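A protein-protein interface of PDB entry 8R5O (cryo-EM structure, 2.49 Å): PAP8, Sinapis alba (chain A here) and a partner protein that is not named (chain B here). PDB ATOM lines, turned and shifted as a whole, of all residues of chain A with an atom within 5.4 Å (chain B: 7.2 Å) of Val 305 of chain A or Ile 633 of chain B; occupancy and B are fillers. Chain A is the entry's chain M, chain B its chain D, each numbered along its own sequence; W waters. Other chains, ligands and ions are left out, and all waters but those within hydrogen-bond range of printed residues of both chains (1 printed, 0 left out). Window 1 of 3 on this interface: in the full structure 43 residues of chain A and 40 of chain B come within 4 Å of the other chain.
Water W1 bridges the backbone carbonyl oxygen (O) of Ile 620 of chain B and the guanidinium group (NH1) of Arg 285 of chain A.
Hydrophobic or aromatic side chains of chain B that line the printed part of chain A: Trp 603, Ile 620, His 623 and Ile 633. Along chain B the printed residues that touch a printed residue of chain A span positions 557 to 635. Hydrophobic or aromatic side chains of chain A that line the printed part of chain B: Val 305 and Ile 306. Among the printed residues, Asp or Glu carboxylates within 4 Å of a Lys or Arg side-chain nitrogen of the other chain: Arg 285 of chain A with Glu 621 of chain B.
The guanidinium group of Arg 285 of chain A is in salt-bridge range of the side-chain carboxylate of Glu 309 of chain A (3.1 Å). The guanidinium group (NH1) of Arg 308 of chain A is in salt-bridge range of the side-chain carboxylate (OD2) of Asp 300 of chain A, 2.7 Å away. O of Ile 633 of chain B sits at hydrogen-bond distance from N of Ile 620 of chain B. A ring nitrogen (NE2) of His 623 of chain B sits at hydrogen-bond distance from the side-chain carboxylate (OE2) of Glu 621 of chain B (2.7 Å). The backbone carbonyl oxygen (O) of His 623 of chain B sits at hydrogen-bond distance from the backbone NH (N) of His 631 of chain B (2.8 Å). The side-chain hydroxyl of Tyr 634 of chain B is in hydrogen-bond range of the side-chain carboxylate of Glu 632 of chain B (3.4 Å).
The guanidinium group of Arg 285 of chain A is in salt-bridge range of the side-chain carboxylate of Glu 621 of chain B (2.4 Å). The indole nitrogen (NE1) of Trp 603 of chain B is in hydrogen-bond range of the side-chain hydroxyl (OG1) of Thr 303 of chain A, at 3.1 Å. O of Pro 557 of chain B lies within hydrogen-bond range of NE of Arg 308 of chain A.
Among the printed residues, pairs that only touch across the chains: Arg 285 of chain A with Ile 620 of chain B, Asp 300 of chain A with His 623 of chain B, Pro 302 of chain A with Ile 633 of chain B, Thr 304 of chain A with Pro 557 of chain B, Val 305 of chain A with Ile 620 of chain B, Val 305 of chain A with Glu 621 of chain B, Val 305 of chain A with Ile 633 of chain B, Ile 306 of chain A with Trp 603 of chain B, Ile 306 of chain A with Ile 633 of chain B, Ile 306 of chain A with Tyr 634 of chain B, Ile 306 of chain A with Ala 635 of chain B and Glu 309 of chain A with Ile 620 of chain B.
Of the printed residues of chain B, Pro 302 of chain A touches Ile 633. Val 305 of chain A touches just these residues of chain B: Ile 620, Glu 621 and Ile 633. Printed residues of chain B within 4 Å of Ile 306 of chain A: Trp 603 (3.6 Å), Ile 633 (3.8 Å), Tyr 634 (3.3 Å) and Ala 635 (3.8 Å). Glu 307 of chain A touches none of the printed residues of chain B. Of the printed residues of chain A, Pro 557 of chain B touches Thr 304 and Arg 308. Of the printed residues of chain A, Ile 620 of chain B touches Arg 285 (3.9 Å), Val 305 (3.97 Å) and Glu 309 (3.5 Å). Tyr 637 of chain B touches none of the printed residues of chain A. The nearest residue of chain A that does not touch Ile 633 of chain B is Asp 301 of chain A (5.1 Å).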
ATOM      1  N   ARG A 285      10.629   0.558  16.846  1.00  0.00           N
ATOM      2  CA  ARG A 285      11.978   0.174  16.457  1.00  0.00           C
ATOM      3  C   ARG A 285      12.935   0.483  17.601  1.00  0.00           C
ATOM      4  O   ARG A 285      12.536   0.999  18.649  1.00  0.00           O
ATOM      5  CB  ARG A 285      12.419   0.895  15.178  1.00  0.00           C
ATOM      6  CG  ARG A 285      11.570   0.605  13.960  1.00  0.00           C
ATOM      7  CD  ARG A 285      12.112   1.308  12.730  1.00  0.00           C
ATOM      8  NE  ARG A 285      12.552   0.359  11.714  1.00  0.00           N
ATOM      9  CZ  ARG A 285      13.807  -0.031  11.544  1.00  0.00           C
ATOM     10  NH1 ARG A 285      14.789   0.450  12.288  1.00  0.00           N
ATOM     11  NH2 ARG A 285      14.085  -0.925  10.600  1.00  0.00           N
ATOM     12  N   ASP A 300       5.070  -1.197   5.477  1.00  0.00           N
ATOM     13  CA  ASP A 300       6.179  -1.847   4.796  1.00  0.00           C
ATOM     14  C   ASP A 300       6.007  -3.361   4.801  1.00  0.00           C
ATOM     15  O   ASP A 300       5.545  -3.949   5.782  1.00  0.00           O
ATOM     16  CB  ASP A 300       7.506  -1.477   5.456  1.00  0.00           C
ATOM     17  CG  ASP A 300       7.907  -0.039   5.194  1.00  0.00           C
ATOM     18  OD1 ASP A 300       7.605   0.474   4.097  1.00  0.00           O
ATOM     19  OD2 ASP A 300       8.525   0.578   6.086  1.00  0.00           O
ATOM     20  N   ASP A 301       6.377  -3.984   3.689  1.00  0.00           N
ATOM     21  CA  ASP A 301       6.403  -5.436   3.611  1.00  0.00           C
ATOM     22  C   ASP A 301       7.412  -5.985   4.618  1.00  0.00           C
ATOM     23  O   ASP A 301       8.479  -5.391   4.811  1.00  0.00           O
ATOM     24  CB  ASP A 301       6.773  -5.869   2.190  1.00  0.00           C
ATOM     25  CG  ASP A 301       6.580  -7.353   1.949  1.00  0.00           C
ATOM     26  OD1 ASP A 301       7.244  -8.171   2.618  1.00  0.00           O
ATOM     27  OD2 ASP A 301       5.758  -7.704   1.079  1.00  0.00           O
ATOM     28  N   PRO A 302       7.104  -7.098   5.291  1.00  0.00           N
ATOM     29  CA  PRO A 302       8.094  -7.692   6.206  1.00  0.00           C
ATOM     30  C   PRO A 302       9.408  -8.043   5.532  1.00  0.00           C
ATOM     31  O   PRO A 302      10.463  -7.940   6.169  1.00  0.00           O
ATOM     32  CB  PRO A 302       7.375  -8.941   6.729  1.00  0.00           C
ATOM     33  CG  PRO A 302       5.934  -8.602   6.630  1.00  0.00           C
ATOM     34  CD  PRO A 302       5.797  -7.768   5.388  1.00  0.00           C
ATOM     35  N   THR A 303       9.378  -8.462   4.265  1.00  0.00           N
ATOM     36  CA  THR A 303      10.619  -8.684   3.531  1.00  0.00           C
ATOM     37  C   THR A 303      11.419  -7.393   3.404  1.00  0.00           C
ATOM     38  O   THR A 303      12.642  -7.391   3.584  1.00  0.00           O
ATOM     39  CB  THR A 303      10.318  -9.262   2.148  1.00  0.00           C
ATOM     40  OG1 THR A 303       9.735 -10.563   2.289  1.00  0.00           O
ATOM     41  CG2 THR A 303      11.588  -9.366   1.322  1.00  0.00           C
ATOM     42  N   THR A 304      10.740  -6.283   3.108  1.00  0.00           N
ATOM     43  CA  THR A 304      11.429  -5.004   2.976  1.00  0.00           C
ATOM     44  C   THR A 304      12.105  -4.605   4.279  1.00  0.00           C
ATOM     45  O   THR A 304      13.238  -4.115   4.273  1.00  0.00           O
ATOM     46  CB  THR A 304      10.445  -3.922   2.530  1.00  0.00           C
ATOM     47  OG1 THR A 304       9.817  -4.322   1.306  1.00  0.00           O
ATOM     48  CG2 THR A 304      11.165  -2.607   2.309  1.00  0.00           C
ATOM     49  N   VAL A 305      11.429  -4.820   5.410  1.00  0.00           N
ATOM     50  CA  VAL A 305      12.006  -4.472   6.706  1.00  0.00           C
ATOM     51  C   VAL A 305      13.273  -5.279   6.956  1.00  0.00           C
ATOM     52  O   VAL A 305      14.299  -4.741   7.389  1.00  0.00           O
ATOM     53  CB  VAL A 305      10.972  -4.684   7.827  1.00  0.00           C
ATOM     54  CG1 VAL A 305      11.596  -4.428   9.185  1.00  0.00           C
ATOM     55  CG2 VAL A 305       9.765  -3.787   7.611  1.00  0.00           C
ATOM     56  N   ILE A 306      13.219  -6.584   6.688  1.00  0.00           N
ATOM     57  CA  ILE A 306      14.377  -7.442   6.918  1.00  0.00           C
ATOM     58  C   ILE A 306      15.512  -7.085   5.968  1.00  0.00           C
ATOM     59  O   ILE A 306      16.675  -6.998   6.376  1.00  0.00           O
ATOM     60  CB  ILE A 306      13.971  -8.922   6.793  1.00  0.00           C
ATOM     61  CG1 ILE A 306      13.004  -9.303   7.915  1.00  0.00           C
ATOM     62  CG2 ILE A 306      15.194  -9.826   6.812  1.00  0.00           C
ATOM     63  CD1 ILE A 306      12.464 -10.704   7.796  1.00  0.00           C
ATOM     64  N   GLU A 307      15.196  -6.861   4.691  1.00  0.00           N
ATOM     65  CA  GLU A 307      16.239  -6.593   3.707  1.00  0.00           C
ATOM     66  C   GLU A 307      16.877  -5.223   3.903  1.00  0.00           C
ATOM     67  O   GLU A 307      18.054  -5.043   3.575  1.00  0.00           O
ATOM     68  CB  GLU A 307      15.674  -6.725   2.295  1.00  0.00           C
ATOM     69  CG  GLU A 307      15.409  -8.163   1.892  1.00  0.00           C
ATOM     70  CD  GLU A 307      15.199  -8.324   0.404  1.00  0.00           C
ATOM     71  OE1 GLU A 307      14.487  -7.490  -0.191  1.00  0.00           O
ATOM     72  OE2 GLU A 307      15.754  -9.284  -0.172  1.00  0.00           O
ATOM     73  N   ARG A 308      16.125  -4.247   4.417  1.00  0.00           N
ATOM     74  CA  ARG A 308      16.721  -2.955   4.738  1.00  0.00           C
ATOM     75  C   ARG A 308      17.805  -3.099   5.794  1.00  0.00           C
ATOM     76  O   ARG A 308      18.887  -2.513   5.672  1.00  0.00           O
ATOM     77  CB  ARG A 308      15.651  -1.981   5.223  1.00  0.00           C
ATOM     78  CG  ARG A 308      14.813  -1.376   4.131  1.00  0.00           C
ATOM     79  CD  ARG A 308      13.667  -0.582   4.718  1.00  0.00           C
ATOM     80  NE  ARG A 308      12.807  -0.019   3.685  1.00  0.00           N
ATOM     81  CZ  ARG A 308      11.605   0.490   3.909  1.00  0.00           C
ATOM     82  NH1 ARG A 308      11.079   0.511   5.121  1.00  0.00           N
ATOM     83  NH2 ARG A 308      10.911   0.987   2.889  1.00  0.00           N
ATOM     84  N   GLU A 309      17.529  -3.874   6.844  1.00  0.00           N
ATOM     85  CA  GLU A 309      18.509  -4.064   7.904  1.00  0.00           C
ATOM     86  C   GLU A 309      19.750  -4.779   7.388  1.00  0.00           C
ATOM     87  O   GLU A 309      20.877  -4.423   7.753  1.00  0.00           O
ATOM     88  CB  GLU A 309      17.876  -4.839   9.060  1.00  0.00           C
ATOM     89  CG  GLU A 309      18.173  -4.263  10.434  1.00  0.00           C
ATOM     90  CD  GLU A 309      17.514  -2.914  10.663  1.00  0.00           C
ATOM     91  OE1 GLU A 309      16.571  -2.570   9.921  1.00  0.00           O
ATOM     92  OE2 GLU A 309      17.942  -2.193  11.591  1.00  0.00           O
ATOM     93  N   PRO B 557      17.043  -1.008  -0.432  1.00  0.00           N
ATOM     94  CA  PRO B 557      15.575  -0.958  -0.455  1.00  0.00           C
ATOM     95  C   PRO B 557      15.015   0.106   0.475  1.00  0.00           C
ATOM     96  O   PRO B 557      14.175  -0.196   1.328  1.00  0.00           O
ATOM     97  CB  PRO B 557      15.165  -2.367   0.001  1.00  0.00           C
ATOM     98  CG  PRO B 557      16.408  -3.203  -0.105  1.00  0.00           C
ATOM     99  CD  PRO B 557      17.543  -2.271   0.132  1.00  0.00           C
ATOM    100  N   TRP B 603       8.783 -17.625   2.629  1.00  0.00           N
ATOM    101  CA  TRP B 603       8.118 -17.651   3.923  1.00  0.00           C
ATOM    102  C   TRP B 603       7.367 -18.963   4.068  1.00  0.00           C
ATOM    103  O   TRP B 603       6.646 -19.375   3.154  1.00  0.00           O
ATOM    104  CB  TRP B 603       7.161 -16.469   4.074  1.00  0.00           C
ATOM    105  CG  TRP B 603       7.855 -15.155   4.166  1.00  0.00           C
ATOM    106  CD1 TRP B 603       8.077 -14.273   3.153  1.00  0.00           C
ATOM    107  CD2 TRP B 603       8.430 -14.571   5.340  1.00  0.00           C
ATOM    108  NE1 TRP B 603       8.749 -13.171   3.622  1.00  0.00           N
ATOM    109  CE2 TRP B 603       8.978 -13.330   4.963  1.00  0.00           C
ATOM    110  CE3 TRP B 603       8.532 -14.976   6.672  1.00  0.00           C
ATOM    111  CZ2 TRP B 603       9.618 -12.492   5.871  1.00  0.00           C
ATOM    112  CZ3 TRP B 603       9.166 -14.145   7.569  1.00  0.00           C
ATOM    113  CH2 TRP B 603       9.701 -12.916   7.167  1.00  0.00           C
ATOM    114  N   VAL B 618      15.700  -8.912  19.777  1.00  0.00           N
ATOM    115  CA  VAL B 618      14.362  -8.324  19.837  1.00  0.00           C
ATOM    116  C   VAL B 618      13.900  -8.044  18.411  1.00  0.00           C
ATOM    117  O   VAL B 618      14.730  -8.047  17.491  1.00  0.00           O
ATOM    118  CB  VAL B 618      14.353  -7.052  20.700  1.00  0.00           C
ATOM    119  CG1 VAL B 618      14.791  -7.371  22.122  1.00  0.00           C
ATOM    120  CG2 VAL B 618      15.231  -5.974  20.080  1.00  0.00           C
ATOM    121  N   PRO B 619      12.606  -7.824  18.168  1.00  0.00           N
ATOM    122  CA  PRO B 619      12.150  -7.591  16.793  1.00  0.00           C
ATOM    123  C   PRO B 619      12.826  -6.383  16.164  1.00  0.00           C
ATOM    124  O   PRO B 619      13.090  -5.377  16.823  1.00  0.00           O
ATOM    125  CB  PRO B 619      10.642  -7.362  16.955  1.00  0.00           C
ATOM    126  CG  PRO B 619      10.293  -8.034  18.221  1.00  0.00           C
ATOM    127  CD  PRO B 619      11.476  -7.870  19.113  1.00  0.00           C
ATOM    128  N   ILE B 620      13.117  -6.503  14.868  1.00  0.00           N
ATOM    129  CA  ILE B 620      13.595  -5.357  14.102  1.00  0.00           C
ATOM    130  C   ILE B 620      12.538  -4.265  14.084  1.00  0.00           C
ATOM    131  O   ILE B 620      12.843  -3.077  14.250  1.00  0.00           O
ATOM    132  CB  ILE B 620      13.976  -5.791  12.675  1.00  0.00           C
ATOM    133  CG1 ILE B 620      14.997  -6.926  12.709  1.00  0.00           C
ATOM    134  CG2 ILE B 620      14.503  -4.607  11.880  1.00  0.00           C
ATOM    135  CD1 ILE B 620      15.216  -7.574  11.365  1.00  0.00           C
ATOM    136  N   GLU B 621      11.282  -4.648  13.889  1.00  0.00           N
ATOM    137  CA  GLU B 621      10.190  -3.701  13.757  1.00  0.00           C
ATOM    138  C   GLU B 621       8.909  -4.366  14.237  1.00  0.00           C
ATOM    139  O   GLU B 621       8.711  -5.565  14.030  1.00  0.00           O
ATOM    140  CB  GLU B 621      10.056  -3.241  12.302  1.00  0.00           C
ATOM    141  CG  GLU B 621       9.361  -1.921  12.105  1.00  0.00           C
ATOM    142  CD  GLU B 621       9.779  -1.244  10.813  1.00  0.00           C
ATOM    143  OE1 GLU B 621      10.998  -1.141  10.564  1.00  0.00           O
ATOM    144  OE2 GLU B 621       8.892  -0.821  10.043  1.00  0.00           O
ATOM    145  N   VAL B 622       8.055  -3.589  14.894  1.00  0.00           N
ATOM    146  CA  VAL B 622       6.734  -4.043  15.312  1.00  0.00           C
ATOM    147  C   VAL B 622       5.708  -3.148  14.639  1.00  0.00           C
ATOM    148  O   VAL B 622       5.729  -1.925  14.823  1.00  0.00           O
ATOM    149  CB  VAL B 622       6.569  -4.018  16.839  1.00  0.00           C
ATOM    150  CG1 VAL B 622       5.132  -4.340  17.223  1.00  0.00           C
ATOM    151  CG2 VAL B 622       7.524  -4.995  17.495  1.00  0.00           C
ATOM    152  N   HIS B 623       4.815  -3.752  13.861  1.00  0.00           N
ATOM    153  CA  HIS B 623       3.734  -3.032  13.199  1.00  0.00           C
ATOM    154  C   HIS B 623       2.457  -3.283  13.988  1.00  0.00           C
ATOM    155  O   HIS B 623       1.953  -4.409  14.026  1.00  0.00           O
ATOM    156  CB  HIS B 623       3.592  -3.474  11.745  1.00  0.00           C
ATOM    157  CG  HIS B 623       4.767  -3.115  10.891  1.00  0.00           C
ATOM    158  ND1 HIS B 623       4.922  -3.577   9.602  1.00  0.00           N
ATOM    159  CD2 HIS B 623       5.844  -2.335  11.142  1.00  0.00           C
ATOM    160  CE1 HIS B 623       6.044  -3.100   9.097  1.00  0.00           C
ATOM    161  NE2 HIS B 623       6.623  -2.344  10.011  1.00  0.00           N
ATOM    162  N   HIS B 631       2.224  -7.141  14.328  1.00  0.00           N
ATOM    163  CA  HIS B 631       3.153  -8.037  13.649  1.00  0.00           C
ATOM    164  C   HIS B 631       4.556  -7.771  14.171  1.00  0.00           C
ATOM    165  O   HIS B 631       5.023  -6.628  14.146  1.00  0.00           O
ATOM    166  CB  HIS B 631       3.116  -7.836  12.134  1.00  0.00           C
ATOM    167  CG  HIS B 631       1.828  -8.242  11.491  1.00  0.00           C
ATOM    168  ND1 HIS B 631       0.678  -8.486  12.211  1.00  0.00           N
ATOM    169  CD2 HIS B 631       1.510  -8.449  10.192  1.00  0.00           C
ATOM    170  CE1 HIS B 631      -0.293  -8.822  11.382  1.00  0.00           C
ATOM    171  NE2 HIS B 631       0.186  -8.811  10.152  1.00  0.00           N
ATOM    172  N   GLU B 632       5.226  -8.819  14.633  1.00  0.00           N
ATOM    173  CA  GLU B 632       6.598  -8.723  15.119  1.00  0.00           C
ATOM    174  C   GLU B 632       7.522  -9.304  14.057  1.00  0.00           C
ATOM    175  O   GLU B 632       7.473 -10.504  13.770  1.00  0.00           O
ATOM    176  CB  GLU B 632       6.757  -9.447  16.452  1.00  0.00           C
ATOM    177  CG  GLU B 632       5.982  -8.810  17.587  1.00  0.00           C
ATOM    178  CD  GLU B 632       6.126  -9.568  18.888  1.00  0.00           C
ATOM    179  OE1 GLU B 632       6.240 -10.811  18.846  1.00  0.00           O
ATOM    180  OE2 GLU B 632       6.133  -8.921  19.955  1.00  0.00           O
ATOM    181  N   ILE B 633       8.363  -8.454  13.481  1.00  0.00           N
ATOM    182  CA  ILE B 633       9.249  -8.836  12.388  1.00  0.00           C
ATOM    183  C   ILE B 633      10.639  -9.050  12.970  1.00  0.00           C
ATOM    184  O   ILE B 633      11.302  -8.099  13.393  1.00  0.00           O
ATOM    185  CB  ILE B 633       9.260  -7.777  11.279  1.00  0.00           C
ATOM    186  CG1 ILE B 633       7.846  -7.568  10.735  1.00  0.00           C
ATOM    187  CG2 ILE B 633      10.208  -8.183  10.167  1.00  0.00           C
ATOM    188  CD1 ILE B 633       7.716  -6.394   9.800  1.00  0.00           C
ATOM    189  N   TYR B 634      11.078 -10.303  13.000  1.00  0.00           N
ATOM    190  CA  TYR B 634      12.419 -10.654  13.432  1.00  0.00           C
ATOM    191  C   TYR B 634      13.308 -10.847  12.209  1.00  0.00           C
ATOM    192  O   TYR B 634      12.864 -10.759  11.063  1.00  0.00           O
ATOM    193  CB  TYR B 634      12.402 -11.913  14.301  1.00  0.00           C
ATOM    194  CG  TYR B 634      11.656 -11.767  15.605  1.00  0.00           C
ATOM    195  CD1 TYR B 634      10.275 -11.906  15.656  1.00  0.00           C
ATOM    196  CD2 TYR B 634      12.332 -11.505  16.788  1.00  0.00           C
ATOM    197  CE1 TYR B 634       9.591 -11.777  16.842  1.00  0.00           C
ATOM    198  CE2 TYR B 634      11.654 -11.377  17.982  1.00  0.00           C
ATOM    199  CZ  TYR B 634      10.283 -11.514  18.003  1.00  0.00           C
ATOM    200  OH  TYR B 634       9.599 -11.388  19.186  1.00  0.00           O
ATOM    201  N   ALA B 635      14.587 -11.125  12.462  1.00  0.00           N
ATOM    202  CA  ALA B 635      15.530 -11.312  11.366  1.00  0.00           C
ATOM    203  C   ALA B 635      15.206 -12.548  10.536  1.00  0.00           C
ATOM    204  O   ALA B 635      15.514 -12.584   9.340  1.00  0.00           O
ATOM    205  CB  ALA B 635      16.954 -11.396  11.911  1.00  0.00           C
ATOM    206  N   HIS B 636      14.589 -13.564  11.140  1.00  0.00           N
ATOM    207  CA  HIS B 636      14.346 -14.824  10.452  1.00  0.00           C
ATOM    208  C   HIS B 636      12.903 -15.297  10.482  1.00  0.00           C
ATOM    209  O   HIS B 636      12.583 -16.257   9.775  1.00  0.00           O
ATOM    210  CB  HIS B 636      15.232 -15.932  11.037  1.00  0.00           C
ATOM    211  CG  HIS B 636      16.696 -15.644  10.935  1.00  0.00           C
ATOM    212  ND1 HIS B 636      17.543 -15.704  12.020  1.00  0.00           N
ATOM    213  CD2 HIS B 636      17.463 -15.287   9.879  1.00  0.00           C
ATOM    214  CE1 HIS B 636      18.769 -15.399  11.635  1.00  0.00           C
ATOM    215  NE2 HIS B 636      18.747 -15.140  10.341  1.00  0.00           N
ATOM    216  N   TYR B 637      12.025 -14.671  11.260  1.00  0.00           N
ATOM    217  CA  TYR B 637      10.639 -15.105  11.302  1.00  0.00           C
ATOM    218  C   TYR B 637       9.735 -13.928  11.629  1.00  0.00           C
ATOM    219  O   TYR B 637      10.176 -12.898  12.144  1.00  0.00           O
ATOM    220  CB  TYR B 637      10.430 -16.244  12.311  1.00  0.00           C
ATOM    221  CG  TYR B 637      11.183 -16.077  13.608  1.00  0.00           C
ATOM    222  CD1 TYR B 637      10.677 -15.293  14.632  1.00  0.00           C
ATOM    223  CD2 TYR B 637      12.397 -16.713  13.811  1.00  0.00           C
ATOM    224  CE1 TYR B 637      11.365 -15.140  15.819  1.00  0.00           C
ATOM    225  CE2 TYR B 637      13.091 -16.566  14.993  1.00  0.00           C
ATOM    226  CZ  TYR B 637      12.572 -15.779  15.993  1.00  0.00           C
ATOM    227  OH  TYR B 637      13.265 -15.634  17.172  1.00  0.00           O
ATOM    228  N   LEU B 638       8.458 -14.099  11.304  1.00  0.00           N
ATOM    229  CA  LEU B 638       7.412 -13.127  11.589  1.00  0.00           C
ATOM    230  C   LEU B 638       6.377 -13.772  12.495  1.00  0.00           C
ATOM    231  O   LEU B 638       5.944 -14.901  12.244  1.00  0.00           O
ATOM    232  CB  LEU B 638       6.749 -12.636  10.302  1.00  0.00           C
ATOM    233  CG  LEU B 638       5.419 -11.902  10.465  1.00  0.00           C
ATOM    234  CD1 LEU B 638       5.620 -10.526  11.080  1.00  0.00           C
ATOM    235  CD2 LEU B 638       4.710 -11.796   9.129  1.00  0.00           C
ATOM    236  N   ILE B 639       5.979 -13.057  13.541  1.00  0.00           N
ATOM    237  CA  ILE B 639       5.000 -13.543  14.503  1.00  0.00           C
ATOM    238  C   ILE B 639       3.834 -12.569  14.539  1.00  0.00           C
ATOM    239  O   ILE B 639       4.031 -11.362  14.723  1.00  0.00           O
ATOM    240  CB  ILE B 639       5.623 -13.717  15.896  1.00  0.00           C
ATOM    241  CG1 ILE B 639       6.760 -14.731  15.815  1.00  0.00           C
ATOM    242  CG2 ILE B 639       4.576 -14.161  16.900  1.00  0.00           C
ATOM    243  CD1 ILE B 639       7.638 -14.725  17.002  1.00  0.00           C
HETATM  244  O   HOH W   1      14.934  -1.447  15.001  1.00  0.00           O
